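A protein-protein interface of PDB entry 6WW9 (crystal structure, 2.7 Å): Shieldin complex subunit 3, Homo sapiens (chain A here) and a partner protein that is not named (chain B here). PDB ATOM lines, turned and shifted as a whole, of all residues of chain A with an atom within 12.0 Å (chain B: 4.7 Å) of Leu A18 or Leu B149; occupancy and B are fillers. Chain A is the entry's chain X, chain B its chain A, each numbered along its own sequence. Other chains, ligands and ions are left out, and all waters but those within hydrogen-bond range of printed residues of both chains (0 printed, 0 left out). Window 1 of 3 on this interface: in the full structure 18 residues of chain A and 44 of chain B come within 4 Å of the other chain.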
ATOM      1  N   PHE A   9     -16.472  19.262  30.527  1.00  0.00           N
ATOM      2  CA  PHE A   9     -17.116  20.022  29.457  1.00  0.00           C
ATOM      3  C   PHE A   9     -18.477  19.401  29.174  1.00  0.00           C
ATOM      4  O   PHE A   9     -18.600  18.516  28.312  1.00  0.00           O
ATOM      5  CB  PHE A   9     -16.250  20.048  28.201  1.00  0.00           C
ATOM      6  CG  PHE A   9     -14.797  20.310  28.472  1.00  0.00           C
ATOM      7  CD1 PHE A   9     -14.363  21.574  28.833  1.00  0.00           C
ATOM      8  CD2 PHE A   9     -13.863  19.293  28.358  1.00  0.00           C
ATOM      9  CE1 PHE A   9     -13.026  21.818  29.082  1.00  0.00           C
ATOM     10  CE2 PHE A   9     -12.525  19.530  28.604  1.00  0.00           C
ATOM     11  CZ  PHE A   9     -12.106  20.794  28.968  1.00  0.00           C
ATOM     12  N   PRO A  10     -19.524  19.830  29.880  1.00  0.00           N
ATOM     13  CA  PRO A  10     -20.864  19.291  29.625  1.00  0.00           C
ATOM     14  C   PRO A  10     -21.321  19.584  28.203  1.00  0.00           C
ATOM     15  O   PRO A  10     -20.824  20.490  27.532  1.00  0.00           O
ATOM     16  CB  PRO A  10     -21.739  20.018  30.654  1.00  0.00           C
ATOM     17  CG  PRO A  10     -20.787  20.443  31.729  1.00  0.00           C
ATOM     18  CD  PRO A  10     -19.504  20.759  31.022  1.00  0.00           C
ATOM     19  N   TYR A  11     -22.292  18.793  27.747  1.00  0.00           N
ATOM     20  CA  TYR A  11     -22.765  18.903  26.372  1.00  0.00           C
ATOM     21  C   TYR A  11     -23.382  20.274  26.121  1.00  0.00           C
ATOM     22  O   TYR A  11     -24.376  20.642  26.754  1.00  0.00           O
ATOM     23  CB  TYR A  11     -23.776  17.795  26.075  1.00  0.00           C
ATOM     24  CG  TYR A  11     -24.427  17.931  24.719  1.00  0.00           C
ATOM     25  CD1 TYR A  11     -23.659  17.974  23.563  1.00  0.00           C
ATOM     26  CD2 TYR A  11     -25.808  18.017  24.593  1.00  0.00           C
ATOM     27  CE1 TYR A  11     -24.245  18.103  22.321  1.00  0.00           C
ATOM     28  CE2 TYR A  11     -26.406  18.145  23.352  1.00  0.00           C
ATOM     29  CZ  TYR A  11     -25.617  18.186  22.220  1.00  0.00           C
ATOM     30  OH  TYR A  11     -26.199  18.313  20.982  1.00  0.00           O
ATOM     31  N   ASP A  12     -22.785  21.025  25.194  1.00  0.00           N
ATOM     32  CA  ASP A  12     -23.231  22.365  24.818  1.00  0.00           C
ATOM     33  C   ASP A  12     -23.838  22.290  23.421  1.00  0.00           C
ATOM     34  O   ASP A  12     -23.130  22.022  22.445  1.00  0.00           O
ATOM     35  CB  ASP A  12     -22.068  23.359  24.861  1.00  0.00           C
ATOM     36  CG  ASP A  12     -22.509  24.806  24.653  1.00  0.00           C
ATOM     37  OD1 ASP A  12     -23.719  25.061  24.466  1.00  0.00           O
ATOM     38  OD2 ASP A  12     -21.634  25.697  24.682  1.00  0.00           O
ATOM     39  N   GLY A  13     -25.147  22.533  23.325  1.00  0.00           N
ATOM     40  CA  GLY A  13     -25.809  22.512  22.034  1.00  0.00           C
ATOM     41  C   GLY A  13     -25.416  23.653  21.121  1.00  0.00           C
ATOM     42  O   GLY A  13     -25.681  23.585  19.914  1.00  0.00           O
ATOM     43  N   SER A  14     -24.786  24.697  21.665  1.00  0.00           N
ATOM     44  CA  SER A  14     -24.414  25.845  20.847  1.00  0.00           C
ATOM     45  C   SER A  14     -23.169  25.554  20.018  1.00  0.00           C
ATOM     46  O   SER A  14     -23.149  25.797  18.806  1.00  0.00           O
ATOM     47  CB  SER A  14     -24.198  27.074  21.733  1.00  0.00           C
ATOM     48  OG  SER A  14     -23.016  26.950  22.507  1.00  0.00           O
ATOM     49  N   LYS A  15     -22.122  25.031  20.656  1.00  0.00           N
ATOM     50  CA  LYS A  15     -20.843  24.774  19.994  1.00  0.00           C
ATOM     51  C   LYS A  15     -20.860  23.353  19.444  1.00  0.00           C
ATOM     52  O   LYS A  15     -20.495  22.393  20.125  1.00  0.00           O
ATOM     53  CB  LYS A  15     -19.688  24.989  20.964  1.00  0.00           C
ATOM     54  CG  LYS A  15     -18.335  25.157  20.297  1.00  0.00           C
ATOM     55  CD  LYS A  15     -17.212  25.150  21.318  1.00  0.00           C
ATOM     56  CE  LYS A  15     -17.402  26.229  22.369  1.00  0.00           C
ATOM     57  NZ  LYS A  15     -16.329  26.147  23.395  1.00  0.00           N
ATOM     58  N   LEU A  16     -21.289  23.217  18.190  1.00  0.00           N
ATOM     59  CA  LEU A  16     -21.340  21.902  17.562  1.00  0.00           C
ATOM     60  C   LEU A  16     -19.935  21.439  17.179  1.00  0.00           C
ATOM     61  O   LEU A  16     -19.117  22.246  16.728  1.00  0.00           O
ATOM     62  CB  LEU A  16     -22.232  21.929  16.326  1.00  0.00           C
ATOM     63  CG  LEU A  16     -23.732  21.887  16.618  1.00  0.00           C
ATOM     64  CD1 LEU A  16     -24.528  21.939  15.324  1.00  0.00           C
ATOM     65  CD2 LEU A  16     -24.079  20.643  17.427  1.00  0.00           C
ATOM     66  N   PRO A  17     -19.638  20.155  17.336  1.00  0.00           N
ATOM     67  CA  PRO A  17     -18.293  19.645  17.056  1.00  0.00           C
ATOM     68  C   PRO A  17     -18.099  19.368  15.568  1.00  0.00           C
ATOM     69  O   PRO A  17     -19.006  19.523  14.752  1.00  0.00           O
ATOM     70  CB  PRO A  17     -18.245  18.354  17.871  1.00  0.00           C
ATOM     71  CG  PRO A  17     -19.658  17.869  17.854  1.00  0.00           C
ATOM     72  CD  PRO A  17     -20.530  19.103  17.855  1.00  0.00           C
ATOM     73  N   LEU A  18     -16.886  18.946  15.230  1.00  0.00           N
ATOM     74  CA  LEU A  18     -16.513  18.591  13.870  1.00  0.00           C
ATOM     75  C   LEU A  18     -16.590  17.081  13.673  1.00  0.00           C
ATOM     76  O   LEU A  18     -16.381  16.301  14.606  1.00  0.00           O
ATOM     77  CB  LEU A  18     -15.103  19.087  13.551  1.00  0.00           C
ATOM     78  CG  LEU A  18     -14.944  20.605  13.474  1.00  0.00           C
ATOM     79  CD1 LEU A  18     -13.556  21.020  13.928  1.00  0.00           C
ATOM     80  CD2 LEU A  18     -15.210  21.078  12.055  1.00  0.00           C
ATOM     81  N   ARG A  19     -16.882  16.677  12.437  1.00  0.00           N
ATOM     82  CA  ARG A  19     -17.090  15.285  12.069  1.00  0.00           C
ATOM     83  C   ARG A  19     -16.491  15.039  10.690  1.00  0.00           C
ATOM     84  O   ARG A  19     -16.646  15.878   9.791  1.00  0.00           O
ATOM     85  CB  ARG A  19     -18.587  14.941  12.058  1.00  0.00           C
ATOM     86  CG  ARG A  19     -18.921  13.519  11.639  1.00  0.00           C
ATOM     87  CD  ARG A  19     -20.300  13.456  10.995  1.00  0.00           C
ATOM     88  NE  ARG A  19     -20.843  12.099  10.968  1.00  0.00           N
ATOM     89  CZ  ARG A  19     -20.555  11.188  10.042  1.00  0.00           C
ATOM     90  NH1 ARG A  19     -19.717  11.474   9.055  1.00  0.00           N
ATOM     91  NH2 ARG A  19     -21.106   9.983  10.108  1.00  0.00           N
ATOM     92  N   PRO A  20     -15.790  13.921  10.496  1.00  0.00           N
ATOM     93  CA  PRO A  20     -15.272  13.610   9.158  1.00  0.00           C
ATOM     94  C   PRO A  20     -16.406  13.404   8.164  1.00  0.00           C
ATOM     95  O   PRO A  20     -17.401  12.740   8.456  1.00  0.00           O
ATOM     96  CB  PRO A  20     -14.474  12.318   9.374  1.00  0.00           C
ATOM     97  CG  PRO A  20     -14.159  12.300  10.833  1.00  0.00           C
ATOM     98  CD  PRO A  20     -15.334  12.949  11.503  1.00  0.00           C
ATOM     99  N   LYS A  21     -16.250  13.998   6.979  1.00  0.00           N
ATOM    100  CA  LYS A  21     -17.268  13.846   5.944  1.00  0.00           C
ATOM    101  C   LYS A  21     -17.375  12.398   5.487  1.00  0.00           C
ATOM    102  O   LYS A  21     -18.480  11.886   5.272  1.00  0.00           O
ATOM    103  CB  LYS A  21     -16.957  14.765   4.763  1.00  0.00           C
ATOM    104  CG  LYS A  21     -18.003  14.749   3.661  1.00  0.00           C
ATOM    105  CD  LYS A  21     -19.330  15.308   4.145  1.00  0.00           C
ATOM    106  CE  LYS A  21     -20.313  15.459   2.996  1.00  0.00           C
ATOM    107  NZ  LYS A  21     -20.624  14.151   2.358  1.00  0.00           N
ATOM    108  N   ARG A  22     -16.241  11.717   5.344  1.00  0.00           N
ATOM    109  CA  ARG A  22     -16.249  10.320   4.941  1.00  0.00           C
ATOM    110  C   ARG A  22     -16.721   9.434   6.091  1.00  0.00           C
ATOM    111  O   ARG A  22     -16.793   9.848   7.251  1.00  0.00           O
ATOM    112  CB  ARG A  22     -14.859   9.879   4.486  1.00  0.00           C
ATOM    113  CG  ARG A  22     -14.235  10.761   3.423  1.00  0.00           C
ATOM    114  CD  ARG A  22     -13.754   9.928   2.250  1.00  0.00           C
ATOM    115  NE  ARG A  22     -12.962  10.710   1.306  1.00  0.00           N
ATOM    116  CZ  ARG A  22     -13.476  11.504   0.372  1.00  0.00           C
ATOM    117  NH1 ARG A  22     -14.792  11.633   0.253  1.00  0.00           N
ATOM    118  NH2 ARG A  22     -12.674  12.173  -0.444  1.00  0.00           N
ATOM    119  N   SER A  23     -17.040   8.186   5.751  1.00  0.00           N
ATOM    120  CA  SER A  23     -17.451   7.186   6.718  1.00  0.00           C
ATOM    121  C   SER A  23     -16.483   6.008   6.697  1.00  0.00           C
ATOM    122  O   SER A  23     -15.918   5.683   5.647  1.00  0.00           O
ATOM    123  CB  SER A  23     -18.873   6.689   6.428  1.00  0.00           C
ATOM    124  OG  SER A  23     -19.802   7.757   6.495  1.00  0.00           O
ATOM    125  N   PRO A  24     -16.261   5.361   7.837  1.00  0.00           N
ATOM    126  CA  PRO A  24     -15.359   4.209   7.873  1.00  0.00           C
ATOM    127  C   PRO A  24     -15.944   3.043   7.099  1.00  0.00           C
ATOM    128  O   PRO A  24     -17.156   3.011   6.836  1.00  0.00           O
ATOM    129  CB  PRO A  24     -15.252   3.891   9.372  1.00  0.00           C
ATOM    130  CG  PRO A  24     -16.517   4.414   9.946  1.00  0.00           C
ATOM    131  CD  PRO A  24     -16.824   5.658   9.165  1.00  0.00           C
ATOM    132  N   LYS B  82     -12.660  18.000  23.740  1.00  0.00           N
ATOM    133  CA  LYS B  82     -13.106  16.619  23.761  1.00  0.00           C
ATOM    134  C   LYS B  82     -12.867  15.973  22.407  1.00  0.00           C
ATOM    135  O   LYS B  82     -13.071  16.600  21.363  1.00  0.00           O
ATOM    136  CB  LYS B  82     -14.599  16.516  24.106  1.00  0.00           C
ATOM    137  CG  LYS B  82     -14.960  17.018  25.488  1.00  0.00           C
ATOM    138  CD  LYS B  82     -16.231  17.847  25.448  1.00  0.00           C
ATOM    139  CE  LYS B  82     -17.406  17.041  24.932  1.00  0.00           C
ATOM    140  NZ  LYS B  82     -18.662  17.837  24.978  1.00  0.00           N
ATOM    141  N   VAL B  83     -12.431  14.718  22.437  1.00  0.00           N
ATOM    142  CA  VAL B  83     -12.437  13.838  21.278  1.00  0.00           C
ATOM    143  C   VAL B  83     -13.346  12.666  21.617  1.00  0.00           C
ATOM    144  O   VAL B  83     -13.096  11.943  22.589  1.00  0.00           O
ATOM    145  CB  VAL B  83     -11.025  13.360  20.908  1.00  0.00           C
ATOM    146  CG1 VAL B  83     -11.100  12.257  19.871  1.00  0.00           C
ATOM    147  CG2 VAL B  83     -10.201  14.523  20.389  1.00  0.00           C
ATOM    148  N   VAL B  84     -14.404  12.487  20.831  1.00  0.00           N
ATOM    149  CA  VAL B  84     -15.473  11.549  21.153  1.00  0.00           C
ATOM    150  C   VAL B  84     -15.561  10.494  20.057  1.00  0.00           C
ATOM    151  O   VAL B  84     -15.646  10.828  18.870  1.00  0.00           O
ATOM    152  CB  VAL B  84     -16.823  12.273  21.323  1.00  0.00           C
ATOM    153  CG1 VAL B  84     -17.903  11.298  21.773  1.00  0.00           C
ATOM    154  CG2 VAL B  84     -16.692  13.424  22.313  1.00  0.00           C
ATOM    155  N   VAL B  86     -18.098   7.801  18.677  1.00  0.00           N
ATOM    156  CA  VAL B  86     -19.549   7.654  18.726  1.00  0.00           C
ATOM    157  C   VAL B  86     -19.933   6.364  18.018  1.00  0.00           C
ATOM    158  O   VAL B  86     -19.579   6.164  16.851  1.00  0.00           O
ATOM    159  CB  VAL B  86     -20.264   8.853  18.086  1.00  0.00           C
ATOM    160  CG1 VAL B  86     -21.769   8.682  18.178  1.00  0.00           C
ATOM    161  CG2 VAL B  86     -19.826  10.145  18.751  1.00  0.00           C
ATOM    162  N   THR B 147     -18.179   7.037  14.251  1.00  0.00           N
ATOM    163  CA  THR B 147     -17.584   8.270  13.759  1.00  0.00           C
ATOM    164  C   THR B 147     -16.873   8.941  14.926  1.00  0.00           C
ATOM    165  O   THR B 147     -17.042   8.557  16.087  1.00  0.00           O
ATOM    166  CB  THR B 147     -18.633   9.204  13.139  1.00  0.00           C
ATOM    167  OG1 THR B 147     -17.977  10.313  12.510  1.00  0.00           O
ATOM    168  CG2 THR B 147     -19.582   9.729  14.206  1.00  0.00           C
ATOM    169  N   VAL B 148     -16.068   9.951  14.607  1.00  0.00           N
ATOM    170  CA  VAL B 148     -15.281  10.671  15.600  1.00  0.00           C
ATOM    171  C   VAL B 148     -15.760  12.114  15.643  1.00  0.00           C
ATOM    172  O   VAL B 148     -15.866  12.770  14.600  1.00  0.00           O
ATOM    173  CB  VAL B 148     -13.775  10.597  15.287  1.00  0.00           C
ATOM    174  CG1 VAL B 148     -12.982  11.410  16.296  1.00  0.00           C
ATOM    175  CG2 VAL B 148     -13.314   9.151  15.286  1.00  0.00           C
ATOM    176  N   LEU B 149     -16.059  12.600  16.843  1.00  0.00           N
ATOM    177  CA  LEU B 149     -16.439  13.989  17.062  1.00  0.00           C
ATOM    178  C   LEU B 149     -15.290  14.713  17.751  1.00  0.00           C
ATOM    179  O   LEU B 149     -14.735  14.211  18.735  1.00  0.00           O
ATOM    180  CB  LEU B 149     -17.712  14.087  17.907  1.00  0.00           C
ATOM    181  CG  LEU B 149     -19.006  13.494  17.345  1.00  0.00           C
ATOM    182  CD1 LEU B 149     -20.162  13.733  18.312  1.00  0.00           C
ATOM    183  CD2 LEU B 149     -19.321  14.070  15.971  1.00  0.00           C
ATOM    184  N   VAL B 150     -14.935  15.886  17.233  1.00  0.00           N
ATOM    185  CA  VAL B 150     -13.859  16.701  17.786  1.00  0.00           C
ATOM    186  C   VAL B 150     -14.464  18.004  18.286  1.00  0.00           C
ATOM    187  O   VAL B 150     -15.047  18.767  17.504  1.00  0.00           O
ATOM    188  CB  VAL B 150     -12.753  16.969  16.753  1.00  0.00           C
ATOM    189  CG1 VAL B 150     -11.634  17.784  17.381  1.00  0.00           C
ATOM    190  CG2 VAL B 150     -12.216  15.659  16.204  1.00  0.00           C
ATOM    191  N   HIS B 151     -14.333  18.256  19.586  1.00  0.00           N
ATOM    192  CA  HIS B 151     -14.829  19.482  20.207  1.00  0.00           C
ATOM    193  C   HIS B 151     -13.649  20.428  20.394  1.00  0.00           C
ATOM    194  O   HIS B 151     -12.871  20.291  21.341  1.00  0.00           O
ATOM    195  CB  HIS B 151     -15.519  19.183  21.534  1.00  0.00           C
ATOM    196  CG  HIS B 151     -16.867  18.554  21.388  1.00  0.00           C
ATOM    197  ND1 HIS B 151     -17.040  17.208  21.146  1.00  0.00           N
ATOM    198  CD2 HIS B 151     -18.111  19.087  21.450  1.00  0.00           C
ATOM    199  CE1 HIS B 151     -18.330  16.938  21.068  1.00  0.00           C
ATOM    200  NE2 HIS B 151     -19.002  18.061  21.247  1.00  0.00           N
ATOM    201  N   THR B 152     -13.518  21.390  19.485  1.00  0.00           N
ATOM    202  CA  THR B 152     -12.460  22.380  19.582  1.00  0.00           C
ATOM    203  C   THR B 152     -12.783  23.408  20.663  1.00  0.00           C
ATOM    204  O   THR B 152     -13.945  23.651  21.001  1.00  0.00           O
ATOM    205  CB  THR B 152     -12.252  23.084  18.239  1.00  0.00           C
ATOM    206  OG1 THR B 152     -13.471  23.721  17.839  1.00  0.00           O
ATOM    207  CG2 THR B 152     -11.834  22.087  17.170  1.00  0.00           C
ATOM    208  N   ALA B 156     -15.860  25.856  16.297  1.00  0.00           N
ATOM    209  CA  ALA B 156     -15.450  25.364  14.987  1.00  0.00           C
ATOM    210  C   ALA B 156     -15.980  26.245  13.864  1.00  0.00           C
ATOM    211  O   ALA B 156     -15.337  26.366  12.815  1.00  0.00           O
ATOM    212  CB  ALA B 156     -15.920  23.923  14.802  1.00  0.00           C
ATOM    213  N   MET B 160     -13.339  27.107  10.078  1.00  0.00           N
ATOM    214  CA  MET B 160     -13.546  25.738   9.621  1.00  0.00           C
ATOM    215  C   MET B 160     -12.332  25.161   8.905  1.00  0.00           C
ATOM    216  O   MET B 160     -12.229  23.936   8.782  1.00  0.00           O
ATOM    217  CB  MET B 160     -14.766  25.677   8.698  1.00  0.00           C
ATOM    218  CG  MET B 160     -16.089  25.887   9.409  1.00  0.00           C
ATOM    219  SD  MET B 160     -16.566  24.427  10.348  1.00  0.00           S
ATOM    220  CE  MET B 160     -16.721  23.233   9.022  1.00  0.00           C
ATOM    221  N   ILE B 163      -9.002  22.494  10.483  1.00  0.00           N
ATOM    222  CA  ILE B 163      -8.953  21.036  10.545  1.00  0.00           C
ATOM    223  C   ILE B 163      -8.827  20.404   9.165  1.00  0.00           C
ATOM    224  O   ILE B 163      -8.590  19.188   9.071  1.00  0.00           O
ATOM    225  CB  ILE B 163     -10.192  20.481  11.287  1.00  0.00           C
ATOM    226  CG1 ILE B 163      -9.911  19.097  11.889  1.00  0.00           C
ATOM    227  CG2 ILE B 163     -11.393  20.437  10.360  1.00  0.00           C
ATOM    228  CD1 ILE B 163     -10.994  18.616  12.843  1.00  0.00           C
ATOM    229  N   TRP B 171     -13.695  17.635   6.614  1.00  0.00           N
ATOM    230  CA  TRP B 171     -14.479  17.619   7.837  1.00  0.00           C
ATOM    231  C   TRP B 171     -15.662  18.567   7.698  1.00  0.00           C
ATOM    232  O   TRP B 171     -15.576  19.600   7.029  1.00  0.00           O
ATOM    233  CB  TRP B 171     -13.641  18.039   9.047  1.00  0.00           C
ATOM    234  CG  TRP B 171     -12.540  17.097   9.409  1.00  0.00           C
ATOM    235  CD1 TRP B 171     -11.408  16.841   8.693  1.00  0.00           C
ATOM    236  CD2 TRP B 171     -12.449  16.307  10.600  1.00  0.00           C
ATOM    237  NE1 TRP B 171     -10.625  15.928   9.357  1.00  0.00           N
ATOM    238  CE2 TRP B 171     -11.241  15.585  10.531  1.00  0.00           C
ATOM    239  CE3 TRP B 171     -13.276  16.134  11.714  1.00  0.00           C
ATOM    240  CZ2 TRP B 171     -10.840  14.706  11.534  1.00  0.00           C
ATOM    241  CZ3 TRP B 171     -12.876  15.262  12.709  1.00  0.00           C
ATOM    242  CH2 TRP B 171     -11.668  14.558  12.612  1.00  0.00           C
ATOM    243  N   ILE B 172     -16.772  18.207   8.342  1.00  0.00           N
ATOM    244  CA  ILE B 172     -17.960  19.046   8.379  1.00  0.00           C
ATOM    245  C   ILE B 172     -18.420  19.165   9.824  1.00  0.00           C
ATOM    246  O   ILE B 172     -17.998  18.409  10.702  1.00  0.00           O
ATOM    247  CB  ILE B 172     -19.103  18.492   7.499  1.00  0.00           C
ATOM    248  CG1 ILE B 172     -19.610  17.160   8.056  1.00  0.00           C
ATOM    249  CG2 ILE B 172     -18.644  18.335   6.057  1.00  0.00           C
ATOM    250  CD1 ILE B 172     -20.824  16.619   7.332  1.00  0.00           C
ATOM    251  N   LEU B 173     -19.293  20.138  10.067  1.00  0.00           N
ATOM    252  CA  LEU B 173     -19.927  20.246  11.372  1.00  0.00           C
ATOM    253  C   LEU B 173     -20.927  19.116  11.554  1.00  0.00           C
ATOM    254  O   LEU B 173     -21.743  18.845  10.667  1.00  0.00           O
ATOM    255  CB  LEU B 173     -20.637  21.590  11.519  1.00  0.00           C
ATOM    256  CG  LEU B 173     -19.831  22.798  11.986  1.00  0.00           C
ATOM    257  CD1 LEU B 173     -20.782  23.923  12.347  1.00  0.00           C
ATOM    258  CD2 LEU B 173     -18.955  22.436  13.169  1.00  0.00           C
ATOM    259  N   ALA B 174     -20.859  18.448  12.699  1.00  0.00           N
ATOM    260  CA  ALA B 174     -21.921  17.529  13.059  1.00  0.00           C
ATOM    261  C   ALA B 174     -23.176  18.313  13.426  1.00  0.00           C
ATOM    262  O   ALA B 174     -23.122  19.498  13.764  1.00  0.00           O
ATOM    263  CB  ALA B 174     -21.494  16.632  14.221  1.00  0.00           C
ATOM    264  N   ASP B 178     -26.265  13.384  14.988  1.00  0.00           N
ATOM    265  CA  ASP B 178     -25.011  12.669  15.207  1.00  0.00           C
ATOM    266  C   ASP B 178     -24.519  12.756  16.647  1.00  0.00           C
ATOM    267  O   ASP B 178     -23.628  11.985  17.023  1.00  0.00           O
ATOM    268  CB  ASP B 178     -23.898  13.201  14.289  1.00  0.00           C
ATOM    269  CG  ASP B 178     -24.207  13.036  12.807  1.00  0.00           C
ATOM    270  OD1 ASP B 178     -23.945  13.988  12.039  1.00  0.00           O
ATOM    271  OD2 ASP B 178     -24.703  11.964  12.408  1.00  0.00           O
ATOM    272  N   VAL B 179     -25.063  13.671  17.453  1.00  0.00           N
ATOM    273  CA  VAL B 179     -24.470  14.011  18.742  1.00  0.00           C
ATOM    274  C   VAL B 179     -25.432  13.786  19.904  1.00  0.00           C
ATOM    275  O   VAL B 179     -25.010  13.386  20.993  1.00  0.00           O
ATOM    276  CB  VAL B 179     -23.978  15.472  18.742  1.00  0.00           C
ATOM    277  CG1 VAL B 179     -23.098  15.744  19.964  1.00  0.00           C
ATOM    278  CG2 VAL B 179     -23.235  15.781  17.455  1.00  0.00           C
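Printed residues of chain B within 4 Å of Tyr A11: Val B179 (3.5 Å).
Of the printed residues of chain B, Leu A18 touches Val B148, Leu B149, Val B150, Thr B152, Ala B156, Met B160, Ile B163, Trp B171 and Ile B172.
Of the printed residues of chain B, Pro A20 touches Thr B147 (3.9 Å), Val B148 (3.1 Å) and Trp B171 (3.6 Å).
Printed residues of chain B within 4 Å of Lys A21: Ile B172.
No residue of chain A comes within 4 Å of Val B83.
No residue of chain A comes within 4 Å of Val B86.
Val B148 touches three residues of chain A.
Of chain A, only Leu A18 (3.4 Å) comes within 4 Å of Leu B149.
Printed residues of chain A within 4 Å of Val B150: Pro A17 (3.2 Å) and Leu A18 (2.9 Å).
Of chain A, only Lys A15 and Leu A18 come within 4 Å of Thr B152.
Of chain A, only Leu A18 comes within 4 Å of Ala B156.
Of chain A, only Leu A18 (3.7 Å) comes within 4 Å of Ile B163.
Of the printed residues of chain A, Ile B172 touches Leu A18 (3.5 Å), Arg A19 (2.7 Å) and Lys A21 (3.6 Å).
Val B179 touches just one residue of chain A: Tyr A11 (3.5 Å).
The nearest printed residue of chain B that does not touch Leu A18 is Leu B173 (4.1 Å).
The nearest residue of chain A that does not touch Leu B149 is Arg A19 (4.1 Å).
The backbone carbonyl oxygen (O) of Lys B82 sits at hydrogen-bond distance from the backbone NH (N) of His B151 (2.7 Å).
N of Leu B149 sits at hydrogen-bond distance from O of Val B84 (2.7 Å).
The backbone NH (N) of Val B86 lies within hydrogen-bond range of the backbone carbonyl oxygen (O) of Thr B147, 2.9 Å away.
The side-chain amino group (NZ) of Lys B82 is in hydrogen-bond range of the backbone carbonyl oxygen (O) of Phe A9 (3.4 Å).
O of Val B150 lies within hydrogen-bond range of N of Leu A18, 2.9 Å away.
O of Ile B172 lies within hydrogen-bond range of N of Arg A19 (2.7 Å).
The backbone NH (N) of Ala B174 sits at hydrogen-bond distance from the backbone carbonyl oxygen (O) of Pro A17, 3.0 Å away.
The guanidinium group (NE) of Arg A19 is in salt-bridge range of the side-chain carboxylate (OD1) of Asp B178 (3.8 Å).
O of Val B150 touches CB of Pro A17, at 3.2 Å.
Pro A17 touches His B151 (CG to NE2, 3.5 Å).
CD2 of Leu B173 touches O of Pro A17, 3.3 Å away.
O of Leu A18 touches O of Val B148, at 3.6 Å.
Leu A18 touches Thr B152.
Ile B163 touches Leu A18 (CD1 to CD1, 3.7 Å).
O of Arg A19 touches CA of Trp B171, at 3.4 Å.
Val B148 touches Pro A20.
Pro A20 touches Trp B171 (N to CE3, 3.6 Å).
CG2 of Ile B172 touches CD of Lys A21 (3.6 Å).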
